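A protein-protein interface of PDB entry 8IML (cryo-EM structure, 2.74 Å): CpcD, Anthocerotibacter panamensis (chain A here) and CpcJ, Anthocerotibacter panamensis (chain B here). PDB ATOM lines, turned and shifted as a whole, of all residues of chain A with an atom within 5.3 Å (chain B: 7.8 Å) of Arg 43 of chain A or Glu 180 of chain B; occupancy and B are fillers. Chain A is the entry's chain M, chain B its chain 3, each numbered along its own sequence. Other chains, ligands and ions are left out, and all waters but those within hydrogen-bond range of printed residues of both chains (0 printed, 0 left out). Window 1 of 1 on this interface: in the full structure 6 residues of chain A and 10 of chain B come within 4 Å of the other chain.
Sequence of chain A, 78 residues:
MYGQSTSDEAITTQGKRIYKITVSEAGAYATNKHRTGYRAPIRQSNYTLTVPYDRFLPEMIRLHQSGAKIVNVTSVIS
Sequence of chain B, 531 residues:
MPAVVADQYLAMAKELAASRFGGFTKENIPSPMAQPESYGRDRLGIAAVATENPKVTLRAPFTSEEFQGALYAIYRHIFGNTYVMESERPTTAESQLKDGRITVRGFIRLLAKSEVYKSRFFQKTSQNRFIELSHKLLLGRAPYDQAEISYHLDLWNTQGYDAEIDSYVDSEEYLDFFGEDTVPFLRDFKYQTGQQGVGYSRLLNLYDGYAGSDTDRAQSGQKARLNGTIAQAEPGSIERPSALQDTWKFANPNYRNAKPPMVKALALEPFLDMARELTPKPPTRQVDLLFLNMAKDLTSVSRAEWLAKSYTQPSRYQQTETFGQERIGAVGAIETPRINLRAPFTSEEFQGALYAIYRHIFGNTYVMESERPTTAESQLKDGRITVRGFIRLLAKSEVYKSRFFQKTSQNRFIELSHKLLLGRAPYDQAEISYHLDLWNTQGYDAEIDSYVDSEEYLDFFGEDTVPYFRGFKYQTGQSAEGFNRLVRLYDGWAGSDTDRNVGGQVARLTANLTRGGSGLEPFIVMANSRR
The guanidinium group (NH1) of Arg 105 of chain B is in salt-bridge range of the side-chain carboxylate (OE1) of Glu 59 of chain A. The guanidinium group (NH2) of Arg 62 of chain A is in salt-bridge range of the side-chain carboxylate (OE2) of Glu 180 of chain B (3.9 Å). NE of Arg 43 of chain A is in salt-bridge range of OD2 of Asp 181 of chain B, at 2.8 Å. The guanidinium group of Arg 43 of chain A sits close to the guanidinium group of Arg 59 of chain B (3.0 Å). The guanidinium group of Arg 62 of chain A lies close to the guanidinium group of Arg 105 of chain B (3.3 Å).
The backbone NH (N) of Leu 58 of chain B is in hydrogen-bond range of the backbone carbonyl oxygen (O) of Asp 181 of chain B. The side-chain carboxylate (OD2) of Asp 181 of chain B is in salt-bridge range of the guanidinium group (NH2) of Arg 59 of chain B (2.5 Å). OE1 of Glu 180 of chain B sits at hydrogen-bond distance from OG1 of Thr 103 of chain B (3.0 Å). The guanidinium group (NH2) of Arg 105 of chain B is in hydrogen-bond range of the backbone carbonyl oxygen (O) of Val 169 of chain B, at 3.3 Å. The guanidinium group of Arg 62 of chain A lies within salt-bridge range of the side-chain carboxylate of Glu 59 of chain A.
Among the printed residues, pairs that only touch across the chains: Arg 43 of chain A with Glu 180 of chain B, Arg 62 of chain A with Leu 175 of chain B and Pro 41 of chain A with Thr 57 of chain B.
Of chain B, only Arg 59 (3.0 Å), Glu 180 (3.3 Å) and Asp 181 (2.8 Å) come within 4 Å of Arg 43 of chain A. Of the printed residues of chain B, Arg 62 of chain A touches Arg 105 (3.3 Å), Leu 175 (3.4 Å) and Glu 180 (3.9 Å). Printed residues of chain A within 4 Å of Leu 175 of chain B: Arg 62 (3.4 Å). Printed residues of chain A within 4 Å of Arg 105 of chain B: Glu 59 and Arg 62. Of the printed residues of chain B, Pro 41 of chain A touches Thr 57. Of the printed residues of chain B, Glu 59 of chain A touches Arg 105 (3.1 Å). Phe 107 of chain B touches none of the printed residues of chain A. The nearest printed residue of chain A that does not touch Thr 57 of chain B is Arg 43 of chain A (6.5 Å).
Printed residues of chain A that touch a printed residue of chain B: Pro 41, Arg 43, Glu 59 and Arg 62. Along chain A the printed residues that touch a printed residue of chain B span positions 41 to 62. Of the 23 printed residues of chain B, 6 touch a printed residue of chain A. Hydrophobic or aromatic side chains of chain B within 4 Å of the printed part of chain A: Leu 175. Among the printed residues, 8 pairs touch across the chains. Among the printed residues, Asp or Glu carboxylates within 4 Å of a Lys or Arg side-chain nitrogen of the other chain: Arg 43 of chain A with Asp 181 of chain B, Glu 59 of chain A with Arg 105 of chain B and Arg 62 of chain A with Glu 180 of chain B.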
ATOM      1  N   GLU A  25      16.440 -11.298 -13.536  1.00  0.00           N
ATOM      2  CA  GLU A  25      16.669 -11.603 -12.131  1.00  0.00           C
ATOM      3  C   GLU A  25      18.124 -11.326 -11.771  1.00  0.00           C
ATOM      4  O   GLU A  25      19.029 -11.537 -12.584  1.00  0.00           O
ATOM      5  CB  GLU A  25      16.297 -13.054 -11.831  1.00  0.00           C
ATOM      6  CG  GLU A  25      17.262 -14.089 -12.375  1.00  0.00           C
ATOM      7  CD  GLU A  25      16.609 -15.440 -12.586  1.00  0.00           C
ATOM      8  OE1 GLU A  25      17.257 -16.467 -12.293  1.00  0.00           O
ATOM      9  OE2 GLU A  25      15.446 -15.475 -13.043  1.00  0.00           O
ATOM     10  N   TYR A  38      14.834 -23.896  -4.157  1.00  0.00           N
ATOM     11  CA  TYR A  38      14.206 -24.148  -5.454  1.00  0.00           C
ATOM     12  C   TYR A  38      13.168 -25.256  -5.297  1.00  0.00           C
ATOM     13  O   TYR A  38      13.466 -26.438  -5.471  1.00  0.00           O
ATOM     14  CB  TYR A  38      15.251 -24.526  -6.498  1.00  0.00           C
ATOM     15  CG  TYR A  38      15.902 -23.355  -7.197  1.00  0.00           C
ATOM     16  CD1 TYR A  38      15.159 -22.250  -7.584  1.00  0.00           C
ATOM     17  CD2 TYR A  38      17.258 -23.366  -7.487  1.00  0.00           C
ATOM     18  CE1 TYR A  38      15.752 -21.184  -8.232  1.00  0.00           C
ATOM     19  CE2 TYR A  38      17.859 -22.304  -8.131  1.00  0.00           C
ATOM     20  CZ  TYR A  38      17.103 -21.215  -8.500  1.00  0.00           C
ATOM     21  OH  TYR A  38      17.699 -20.155  -9.142  1.00  0.00           O
ATOM     22  N   PRO A  41      12.247 -25.756 -10.782  1.00  0.00           N
ATOM     23  CA  PRO A  41      13.571 -25.902 -11.401  1.00  0.00           C
ATOM     24  C   PRO A  41      14.222 -24.561 -11.707  1.00  0.00           C
ATOM     25  O   PRO A  41      13.552 -23.555 -11.950  1.00  0.00           O
ATOM     26  CB  PRO A  41      13.278 -26.688 -12.683  1.00  0.00           C
ATOM     27  CG  PRO A  41      11.874 -26.349 -13.012  1.00  0.00           C
ATOM     28  CD  PRO A  41      11.169 -26.188 -11.690  1.00  0.00           C
ATOM     29  N   ILE A  42      15.556 -24.562 -11.686  1.00  0.00           N
ATOM     30  CA  ILE A  42      16.317 -23.346 -11.937  1.00  0.00           C
ATOM     31  C   ILE A  42      16.156 -22.929 -13.392  1.00  0.00           C
ATOM     32  O   ILE A  42      16.106 -23.768 -14.302  1.00  0.00           O
ATOM     33  CB  ILE A  42      17.797 -23.551 -11.565  1.00  0.00           C
ATOM     34  CG1 ILE A  42      18.584 -22.250 -11.747  1.00  0.00           C
ATOM     35  CG2 ILE A  42      18.412 -24.686 -12.373  1.00  0.00           C
ATOM     36  CD1 ILE A  42      19.938 -22.260 -11.092  1.00  0.00           C
ATOM     37  N   ARG A  43      16.066 -21.620 -13.618  1.00  0.00           N
ATOM     38  CA  ARG A  43      15.798 -21.072 -14.937  1.00  0.00           C
ATOM     39  C   ARG A  43      16.775 -19.939 -15.211  1.00  0.00           C
ATOM     40  O   ARG A  43      17.500 -19.486 -14.322  1.00  0.00           O
ATOM     41  CB  ARG A  43      14.348 -20.590 -15.043  1.00  0.00           C
ATOM     42  CG  ARG A  43      13.351 -21.726 -15.187  1.00  0.00           C
ATOM     43  CD  ARG A  43      12.098 -21.463 -14.375  1.00  0.00           C
ATOM     44  NE  ARG A  43      11.405 -20.248 -14.795  1.00  0.00           N
ATOM     45  CZ  ARG A  43      10.538 -19.584 -14.036  1.00  0.00           C
ATOM     46  NH1 ARG A  43      10.255 -20.016 -12.814  1.00  0.00           N
ATOM     47  NH2 ARG A  43       9.952 -18.488 -14.498  1.00  0.00           N
ATOM     48  N   GLN A  44      16.789 -19.481 -16.460  1.00  0.00           N
ATOM     49  CA  GLN A  44      17.714 -18.436 -16.867  1.00  0.00           C
ATOM     50  C   GLN A  44      17.362 -17.106 -16.206  1.00  0.00           C
ATOM     51  O   GLN A  44      16.329 -16.957 -15.547  1.00  0.00           O
ATOM     52  CB  GLN A  44      17.716 -18.283 -18.388  1.00  0.00           C
ATOM     53  CG  GLN A  44      17.914 -19.587 -19.142  1.00  0.00           C
ATOM     54  CD  GLN A  44      19.370 -20.002 -19.216  1.00  0.00           C
ATOM     55  OE1 GLN A  44      20.230 -19.420 -18.556  1.00  0.00           O
ATOM     56  NE2 GLN A  44      19.655 -21.012 -20.029  1.00  0.00           N
ATOM     57  N   SER A  45      18.243 -16.124 -16.401  1.00  0.00           N
ATOM     58  CA  SER A  45      18.114 -14.859 -15.685  1.00  0.00           C
ATOM     59  C   SER A  45      17.031 -13.977 -16.294  1.00  0.00           C
ATOM     60  O   SER A  45      16.080 -13.581 -15.609  1.00  0.00           O
ATOM     61  CB  SER A  45      19.455 -14.127 -15.670  1.00  0.00           C
ATOM     62  OG  SER A  45      19.284 -12.769 -15.303  1.00  0.00           O
ATOM     63  N   TYR A  47      13.962 -12.816 -18.880  1.00  0.00           N
ATOM     64  CA  TYR A  47      12.813 -13.303 -19.629  1.00  0.00           C
ATOM     65  C   TYR A  47      11.744 -12.223 -19.612  1.00  0.00           C
ATOM     66  O   TYR A  47      11.822 -11.265 -18.842  1.00  0.00           O
ATOM     67  CB  TYR A  47      12.275 -14.617 -19.053  1.00  0.00           C
ATOM     68  CG  TYR A  47      11.735 -14.504 -17.648  1.00  0.00           C
ATOM     69  CD1 TYR A  47      12.560 -14.691 -16.551  1.00  0.00           C
ATOM     70  CD2 TYR A  47      10.394 -14.236 -17.420  1.00  0.00           C
ATOM     71  CE1 TYR A  47      12.069 -14.594 -15.268  1.00  0.00           C
ATOM     72  CE2 TYR A  47       9.894 -14.138 -16.140  1.00  0.00           C
ATOM     73  CZ  TYR A  47      10.735 -14.318 -15.067  1.00  0.00           C
ATOM     74  OH  TYR A  47      10.239 -14.225 -13.788  1.00  0.00           O
ATOM     75  N   LEU A  49       7.574 -11.244 -19.427  1.00  0.00           N
ATOM     76  CA  LEU A  49       6.228 -11.604 -19.008  1.00  0.00           C
ATOM     77  C   LEU A  49       5.231 -10.661 -19.667  1.00  0.00           C
ATOM     78  O   LEU A  49       5.380  -9.438 -19.583  1.00  0.00           O
ATOM     79  CB  LEU A  49       6.093 -11.535 -17.484  1.00  0.00           C
ATOM     80  CG  LEU A  49       6.491 -12.783 -16.693  1.00  0.00           C
ATOM     81  CD1 LEU A  49       6.415 -12.516 -15.200  1.00  0.00           C
ATOM     82  CD2 LEU A  49       5.606 -13.958 -17.070  1.00  0.00           C
ATOM     83  N   GLU A  59       1.630  -7.663 -10.833  1.00  0.00           N
ATOM     84  CA  GLU A  59       2.806  -8.304 -11.407  1.00  0.00           C
ATOM     85  C   GLU A  59       4.071  -7.535 -11.057  1.00  0.00           C
ATOM     86  O   GLU A  59       5.077  -8.126 -10.646  1.00  0.00           O
ATOM     87  CB  GLU A  59       2.652  -8.414 -12.921  1.00  0.00           C
ATOM     88  CG  GLU A  59       3.515  -9.473 -13.561  1.00  0.00           C
ATOM     89  CD  GLU A  59       2.858 -10.836 -13.540  1.00  0.00           C
ATOM     90  OE1 GLU A  59       3.575 -11.849 -13.683  1.00  0.00           O
ATOM     91  OE2 GLU A  59       1.619 -10.893 -13.386  1.00  0.00           O
ATOM     92  N   ARG A  62       4.859  -7.953  -7.320  1.00  0.00           N
ATOM     93  CA  ARG A  62       5.415  -9.271  -7.042  1.00  0.00           C
ATOM     94  C   ARG A  62       6.863  -9.377  -7.496  1.00  0.00           C
ATOM     95  O   ARG A  62       7.715  -9.899  -6.765  1.00  0.00           O
ATOM     96  CB  ARG A  62       4.570 -10.335  -7.726  1.00  0.00           C
ATOM     97  CG  ARG A  62       5.142 -11.709  -7.620  1.00  0.00           C
ATOM     98  CD  ARG A  62       4.215 -12.684  -8.269  1.00  0.00           C
ATOM     99  NE  ARG A  62       4.177 -12.514  -9.717  1.00  0.00           N
ATOM    100  CZ  ARG A  62       5.114 -12.953 -10.547  1.00  0.00           C
ATOM    101  NH1 ARG A  62       6.174 -13.596 -10.078  1.00  0.00           N
ATOM    102  NH2 ARG A  62       4.990 -12.755 -11.848  1.00  0.00           N
ATOM    103  N   THR B  57       7.263 -30.328 -16.314  1.00  0.00           N
ATOM    104  CA  THR B  57       7.730 -28.962 -16.494  1.00  0.00           C
ATOM    105  C   THR B  57       7.875 -28.666 -17.978  1.00  0.00           C
ATOM    106  O   THR B  57       8.389 -29.492 -18.737  1.00  0.00           O
ATOM    107  CB  THR B  57       9.060 -28.742 -15.781  1.00  0.00           C
ATOM    108  OG1 THR B  57       8.983 -29.281 -14.457  1.00  0.00           O
ATOM    109  CG2 THR B  57       9.377 -27.271 -15.693  1.00  0.00           C
ATOM    110  N   LEU B  58       7.416 -27.489 -18.390  1.00  0.00           N
ATOM    111  CA  LEU B  58       7.461 -27.069 -19.784  1.00  0.00           C
ATOM    112  C   LEU B  58       8.132 -25.708 -19.867  1.00  0.00           C
ATOM    113  O   LEU B  58       7.701 -24.763 -19.203  1.00  0.00           O
ATOM    114  CB  LEU B  58       6.056 -27.008 -20.380  1.00  0.00           C
ATOM    115  CG  LEU B  58       5.879 -27.309 -21.860  1.00  0.00           C
ATOM    116  CD1 LEU B  58       6.364 -28.698 -22.170  1.00  0.00           C
ATOM    117  CD2 LEU B  58       4.424 -27.162 -22.230  1.00  0.00           C
ATOM    118  N   ARG B  59       9.167 -25.605 -20.694  1.00  0.00           N
ATOM    119  CA  ARG B  59       9.916 -24.372 -20.865  1.00  0.00           C
ATOM    120  C   ARG B  59       9.592 -23.785 -22.240  1.00  0.00           C
ATOM    121  O   ARG B  59       8.704 -24.263 -22.943  1.00  0.00           O
ATOM    122  CB  ARG B  59      11.411 -24.639 -20.673  1.00  0.00           C
ATOM    123  CG  ARG B  59      12.247 -23.405 -20.369  1.00  0.00           C
ATOM    124  CD  ARG B  59      11.556 -22.538 -19.336  1.00  0.00           C
ATOM    125  NE  ARG B  59      12.328 -21.343 -19.013  1.00  0.00           N
ATOM    126  CZ  ARG B  59      11.888 -20.360 -18.234  1.00  0.00           C
ATOM    127  NH1 ARG B  59      12.657 -19.309 -17.987  1.00  0.00           N
ATOM    128  NH2 ARG B  59      10.676 -20.427 -17.702  1.00  0.00           N
ATOM    129  N   LEU B  97       0.370 -21.184 -25.871  1.00  0.00           N
ATOM    130  CA  LEU B  97       1.374 -21.867 -25.066  1.00  0.00           C
ATOM    131  C   LEU B  97       2.531 -22.357 -25.924  1.00  0.00           C
ATOM    132  O   LEU B  97       3.698 -22.224 -25.540  1.00  0.00           O
ATOM    133  CB  LEU B  97       0.735 -23.032 -24.318  1.00  0.00           C
ATOM    134  CG  LEU B  97       1.680 -23.856 -23.449  1.00  0.00           C
ATOM    135  CD1 LEU B  97       2.165 -23.049 -22.278  1.00  0.00           C
ATOM    136  CD2 LEU B  97       1.002 -25.117 -22.995  1.00  0.00           C
ATOM    137  N   ILE B 102       2.245 -17.322 -23.591  1.00  0.00           N
ATOM    138  CA  ILE B 102       1.915 -17.534 -22.191  1.00  0.00           C
ATOM    139  C   ILE B 102       2.809 -18.632 -21.645  1.00  0.00           C
ATOM    140  O   ILE B 102       3.316 -19.477 -22.386  1.00  0.00           O
ATOM    141  CB  ILE B 102       0.432 -17.902 -21.988  1.00  0.00           C
ATOM    142  CG1 ILE B 102       0.016 -19.004 -22.953  1.00  0.00           C
ATOM    143  CG2 ILE B 102      -0.446 -16.692 -22.165  1.00  0.00           C
ATOM    144  CD1 ILE B 102      -1.358 -19.522 -22.694  1.00  0.00           C
ATOM    145  N   THR B 103       3.012 -18.606 -20.335  1.00  0.00           N
ATOM    146  CA  THR B 103       3.683 -19.698 -19.659  1.00  0.00           C
ATOM    147  C   THR B 103       2.668 -20.781 -19.323  1.00  0.00           C
ATOM    148  O   THR B 103       1.475 -20.659 -19.609  1.00  0.00           O
ATOM    149  CB  THR B 103       4.394 -19.194 -18.411  1.00  0.00           C
ATOM    150  OG1 THR B 103       3.524 -18.331 -17.675  1.00  0.00           O
ATOM    151  CG2 THR B 103       5.630 -18.423 -18.794  1.00  0.00           C
ATOM    152  N   VAL B 104       3.143 -21.869 -18.717  1.00  0.00           N
ATOM    153  CA  VAL B 104       2.226 -22.888 -18.222  1.00  0.00           C
ATOM    154  C   VAL B 104       1.311 -22.297 -17.164  1.00  0.00           C
ATOM    155  O   VAL B 104       0.149 -22.693 -17.044  1.00  0.00           O
ATOM    156  CB  VAL B 104       3.017 -24.097 -17.691  1.00  0.00           C
ATOM    157  CG1 VAL B 104       2.096 -25.116 -17.070  1.00  0.00           C
ATOM    158  CG2 VAL B 104       3.799 -24.723 -18.805  1.00  0.00           C
ATOM    159  N   ARG B 105       1.803 -21.318 -16.408  1.00  0.00           N
ATOM    160  CA  ARG B 105       0.951 -20.610 -15.462  1.00  0.00           C
ATOM    161  C   ARG B 105      -0.160 -19.849 -16.172  1.00  0.00           C
ATOM    162  O   ARG B 105      -1.314 -19.864 -15.728  1.00  0.00           O
ATOM    163  CB  ARG B 105       1.792 -19.668 -14.615  1.00  0.00           C
ATOM    164  CG  ARG B 105       0.983 -18.907 -13.604  1.00  0.00           C
ATOM    165  CD  ARG B 105       1.847 -18.279 -12.548  1.00  0.00           C
ATOM    166  NE  ARG B 105       2.415 -17.010 -12.966  1.00  0.00           N
ATOM    167  CZ  ARG B 105       1.995 -15.834 -12.522  1.00  0.00           C
ATOM    168  NH1 ARG B 105       2.565 -14.720 -12.946  1.00  0.00           N
ATOM    169  NH2 ARG B 105       1.015 -15.772 -11.639  1.00  0.00           N
ATOM    170  N   GLY B 106       0.166 -19.170 -17.273  1.00  0.00           N
ATOM    171  CA  GLY B 106      -0.860 -18.476 -18.028  1.00  0.00           C
ATOM    172  C   GLY B 106      -1.868 -19.430 -18.631  1.00  0.00           C
ATOM    173  O   GLY B 106      -3.059 -19.126 -18.715  1.00  0.00           O
ATOM    174  N   PHE B 107      -1.404 -20.604 -19.041  1.00  0.00           N
ATOM    175  CA  PHE B 107      -2.301 -21.629 -19.551  1.00  0.00           C
ATOM    176  C   PHE B 107      -3.239 -22.136 -18.465  1.00  0.00           C
ATOM    177  O   PHE B 107      -4.428 -22.362 -18.716  1.00  0.00           O
ATOM    178  CB  PHE B 107      -1.468 -22.765 -20.128  1.00  0.00           C
ATOM    179  CG  PHE B 107      -2.248 -23.754 -20.913  1.00  0.00           C
ATOM    180  CD1 PHE B 107      -2.868 -23.388 -22.081  1.00  0.00           C
ATOM    181  CD2 PHE B 107      -2.335 -25.060 -20.498  1.00  0.00           C
ATOM    182  CE1 PHE B 107      -3.575 -24.298 -22.801  1.00  0.00           C
ATOM    183  CE2 PHE B 107      -3.036 -25.972 -21.225  1.00  0.00           C
ATOM    184  CZ  PHE B 107      -3.656 -25.592 -22.380  1.00  0.00           C
ATOM    185  N   ILE B 108      -2.721 -22.333 -17.252  1.00  0.00           N
ATOM    186  CA  ILE B 108      -3.570 -22.731 -16.135  1.00  0.00           C
ATOM    187  C   ILE B 108      -4.606 -21.656 -15.858  1.00  0.00           C
ATOM    188  O   ILE B 108      -5.782 -21.951 -15.614  1.00  0.00           O
ATOM    189  CB  ILE B 108      -2.720 -23.016 -14.885  1.00  0.00           C
ATOM    190  CG1 ILE B 108      -1.818 -24.227 -15.102  1.00  0.00           C
ATOM    191  CG2 ILE B 108      -3.599 -23.242 -13.690  1.00  0.00           C
ATOM    192  CD1 ILE B 108      -2.519 -25.419 -15.617  1.00  0.00           C
ATOM    193  N   ARG B 109      -4.183 -20.392 -15.887  1.00  0.00           N
ATOM    194  CA  ARG B 109      -5.111 -19.286 -15.687  1.00  0.00           C
ATOM    195  C   ARG B 109      -6.219 -19.305 -16.726  1.00  0.00           C
ATOM    196  O   ARG B 109      -7.393 -19.108 -16.398  1.00  0.00           O
ATOM    197  CB  ARG B 109      -4.361 -17.962 -15.733  1.00  0.00           C
ATOM    198  CG  ARG B 109      -5.085 -16.821 -15.047  1.00  0.00           C
ATOM    199  CD  ARG B 109      -4.389 -15.508 -15.307  1.00  0.00           C
ATOM    200  NE  ARG B 109      -2.947 -15.658 -15.198  1.00  0.00           N
ATOM    201  CZ  ARG B 109      -2.243 -15.314 -14.127  1.00  0.00           C
ATOM    202  NH1 ARG B 109      -2.851 -14.797 -13.072  1.00  0.00           N
ATOM    203  NH2 ARG B 109      -0.931 -15.494 -14.110  1.00  0.00           N
ATOM    204  N   VAL B 169      -3.940 -18.187  -8.716  1.00  0.00           N
ATOM    205  CA  VAL B 169      -2.760 -18.390  -9.550  1.00  0.00           C
ATOM    206  C   VAL B 169      -1.693 -17.326  -9.309  1.00  0.00           C
ATOM    207  O   VAL B 169      -0.498 -17.615  -9.413  1.00  0.00           O
ATOM    208  CB  VAL B 169      -3.187 -18.457 -11.023  1.00  0.00           C
ATOM    209  CG1 VAL B 169      -2.003 -18.468 -11.906  1.00  0.00           C
ATOM    210  CG2 VAL B 169      -3.968 -19.718 -11.264  1.00  0.00           C
ATOM    211  N   TYR B 174       1.436 -20.421  -4.972  1.00  0.00           N
ATOM    212  CA  TYR B 174       1.455 -21.051  -6.284  1.00  0.00           C
ATOM    213  C   TYR B 174       2.795 -20.851  -6.967  1.00  0.00           C
ATOM    214  O   TYR B 174       3.325 -21.777  -7.584  1.00  0.00           O
ATOM    215  CB  TYR B 174       0.329 -20.484  -7.150  1.00  0.00           C
ATOM    216  CG  TYR B 174       0.271 -21.054  -8.549  1.00  0.00           C
ATOM    217  CD1 TYR B 174       1.100 -20.582  -9.549  1.00  0.00           C
ATOM    218  CD2 TYR B 174      -0.613 -22.064  -8.866  1.00  0.00           C
ATOM    219  CE1 TYR B 174       1.056 -21.102 -10.806  1.00  0.00           C
ATOM    220  CE2 TYR B 174      -0.664 -22.585 -10.130  1.00  0.00           C
ATOM    221  CZ  TYR B 174       0.171 -22.097 -11.093  1.00  0.00           C
ATOM    222  OH  TYR B 174       0.129 -22.610 -12.357  1.00  0.00           O
ATOM    223  N   LEU B 175       3.344 -19.643  -6.901  1.00  0.00           N
ATOM    224  CA  LEU B 175       4.605 -19.381  -7.580  1.00  0.00           C
ATOM    225  C   LEU B 175       5.782 -20.002  -6.853  1.00  0.00           C
ATOM    226  O   LEU B 175       6.768 -20.385  -7.491  1.00  0.00           O
ATOM    227  CB  LEU B 175       4.792 -17.884  -7.750  1.00  0.00           C
ATOM    228  CG  LEU B 175       3.948 -17.422  -8.925  1.00  0.00           C
ATOM    229  CD1 LEU B 175       3.826 -15.950  -8.918  1.00  0.00           C
ATOM    230  CD2 LEU B 175       4.616 -17.875 -10.197  1.00  0.00           C
ATOM    231  N   ASP B 176       5.704 -20.106  -5.527  1.00  0.00           N
ATOM    232  CA  ASP B 176       6.743 -20.795  -4.778  1.00  0.00           C
ATOM    233  C   ASP B 176       6.812 -22.258  -5.169  1.00  0.00           C
ATOM    234  O   ASP B 176       7.902 -22.812  -5.339  1.00  0.00           O
ATOM    235  CB  ASP B 176       6.488 -20.662  -3.281  1.00  0.00           C
ATOM    236  CG  ASP B 176       7.081 -19.403  -2.698  1.00  0.00           C
ATOM    237  OD1 ASP B 176       7.666 -18.605  -3.461  1.00  0.00           O
ATOM    238  OD2 ASP B 176       6.963 -19.207  -1.469  1.00  0.00           O
ATOM    239  N   PHE B 177       5.661 -22.902  -5.332  1.00  0.00           N
ATOM    240  CA  PHE B 177       5.682 -24.337  -5.582  1.00  0.00           C
ATOM    241  C   PHE B 177       5.745 -24.711  -7.054  1.00  0.00           C
ATOM    242  O   PHE B 177       6.326 -25.743  -7.390  1.00  0.00           O
ATOM    243  CB  PHE B 177       4.468 -24.998  -4.938  1.00  0.00           C
ATOM    244  CG  PHE B 177       4.631 -25.231  -3.478  1.00  0.00           C
ATOM    245  CD1 PHE B 177       5.248 -26.372  -3.020  1.00  0.00           C
ATOM    246  CD2 PHE B 177       4.208 -24.290  -2.563  1.00  0.00           C
ATOM    247  CE1 PHE B 177       5.412 -26.582  -1.681  1.00  0.00           C
ATOM    248  CE2 PHE B 177       4.372 -24.495  -1.223  1.00  0.00           C
ATOM    249  CZ  PHE B 177       4.976 -25.641  -0.780  1.00  0.00           C
ATOM    250  N   PHE B 178       5.162 -23.913  -7.944  1.00  0.00           N
ATOM    251  CA  PHE B 178       5.103 -24.255  -9.354  1.00  0.00           C
ATOM    252  C   PHE B 178       5.759 -23.243 -10.278  1.00  0.00           C
ATOM    253  O   PHE B 178       6.053 -23.593 -11.421  1.00  0.00           O
ATOM    254  CB  PHE B 178       3.648 -24.448  -9.800  1.00  0.00           C
ATOM    255  CG  PHE B 178       2.818 -25.220  -8.829  1.00  0.00           C
ATOM    256  CD1 PHE B 178       3.198 -26.479  -8.415  1.00  0.00           C
ATOM    257  CD2 PHE B 178       1.654 -24.691  -8.327  1.00  0.00           C
ATOM    258  CE1 PHE B 178       2.432 -27.184  -7.523  1.00  0.00           C
ATOM    259  CE2 PHE B 178       0.892 -25.395  -7.437  1.00  0.00           C
ATOM    260  CZ  PHE B 178       1.289 -26.641  -7.033  1.00  0.00           C
ATOM    261  N   GLY B 179       5.991 -22.015  -9.833  1.00  0.00           N
ATOM    262  CA  GLY B 179       6.575 -21.039 -10.731  1.00  0.00           C
ATOM    263  C   GLY B 179       5.718 -20.835 -11.961  1.00  0.00           C
ATOM    264  O   GLY B 179       4.488 -20.774 -11.893  1.00  0.00           O
ATOM    265  N   GLU B 180       6.376 -20.741 -13.114  1.00  0.00           N
ATOM    266  CA  GLU B 180       5.689 -20.532 -14.377  1.00  0.00           C
ATOM    267  C   GLU B 180       5.679 -21.749 -15.282  1.00  0.00           C
ATOM    268  O   GLU B 180       4.961 -21.739 -16.283  1.00  0.00           O
ATOM    269  CB  GLU B 180       6.331 -19.373 -15.149  1.00  0.00           C
ATOM    270  CG  GLU B 180       6.656 -18.160 -14.312  1.00  0.00           C
ATOM    271  CD  GLU B 180       5.527 -17.166 -14.272  1.00  0.00           C
ATOM    272  OE1 GLU B 180       4.515 -17.387 -14.969  1.00  0.00           O
ATOM    273  OE2 GLU B 180       5.654 -16.157 -13.552  1.00  0.00           O
ATOM    274  N   ASP B 181       6.444 -22.785 -14.967  1.00  0.00           N
ATOM    275  CA  ASP B 181       6.722 -23.836 -15.934  1.00  0.00           C
ATOM    276  C   ASP B 181       6.256 -25.220 -15.526  1.00  0.00           C
ATOM    277  O   ASP B 181       5.990 -26.042 -16.403  1.00  0.00           O
ATOM    278  CB  ASP B 181       8.219 -23.873 -16.231  1.00  0.00           C
ATOM    279  CG  ASP B 181       8.729 -22.550 -16.738  1.00  0.00           C
ATOM    280  OD1 ASP B 181       8.271 -22.108 -17.812  1.00  0.00           O
ATOM    281  OD2 ASP B 181       9.577 -21.942 -16.061  1.00  0.00           O
ATOM    282  N   THR B 182       6.154 -25.538 -14.243  1.00  0.00           N
ATOM    283  CA  THR B 182       5.712 -26.874 -13.880  1.00  0.00           C
ATOM    284  C   THR B 182       4.223 -26.880 -13.577  1.00  0.00           C
ATOM    285  O   THR B 182       3.690 -25.953 -12.964  1.00  0.00           O
ATOM    286  CB  THR B 182       6.507 -27.446 -12.700  1.00  0.00           C
ATOM    287  OG1 THR B 182       5.991 -28.736 -12.352  1.00  0.00           O
ATOM    288  CG2 THR B 182       6.430 -26.575 -11.509  1.00  0.00           C
ATOM    289  N   VAL B 183       3.556 -27.922 -14.055  1.00  0.00           N
ATOM    290  CA  VAL B 183       2.120 -28.093 -13.832  1.00  0.00           C
ATOM    291  C   VAL B 183       1.866 -28.239 -12.342  1.00  0.00           C
ATOM    292  O   VAL B 183       2.671 -28.882 -11.639  1.00  0.00           O
ATOM    293  CB  VAL B 183       1.611 -29.319 -14.600  1.00  0.00           C
ATOM    294  CG1 VAL B 183       0.096 -29.374 -14.592  1.00  0.00           C
ATOM    295  CG2 VAL B 183       2.151 -29.296 -16.009  1.00  0.00           C
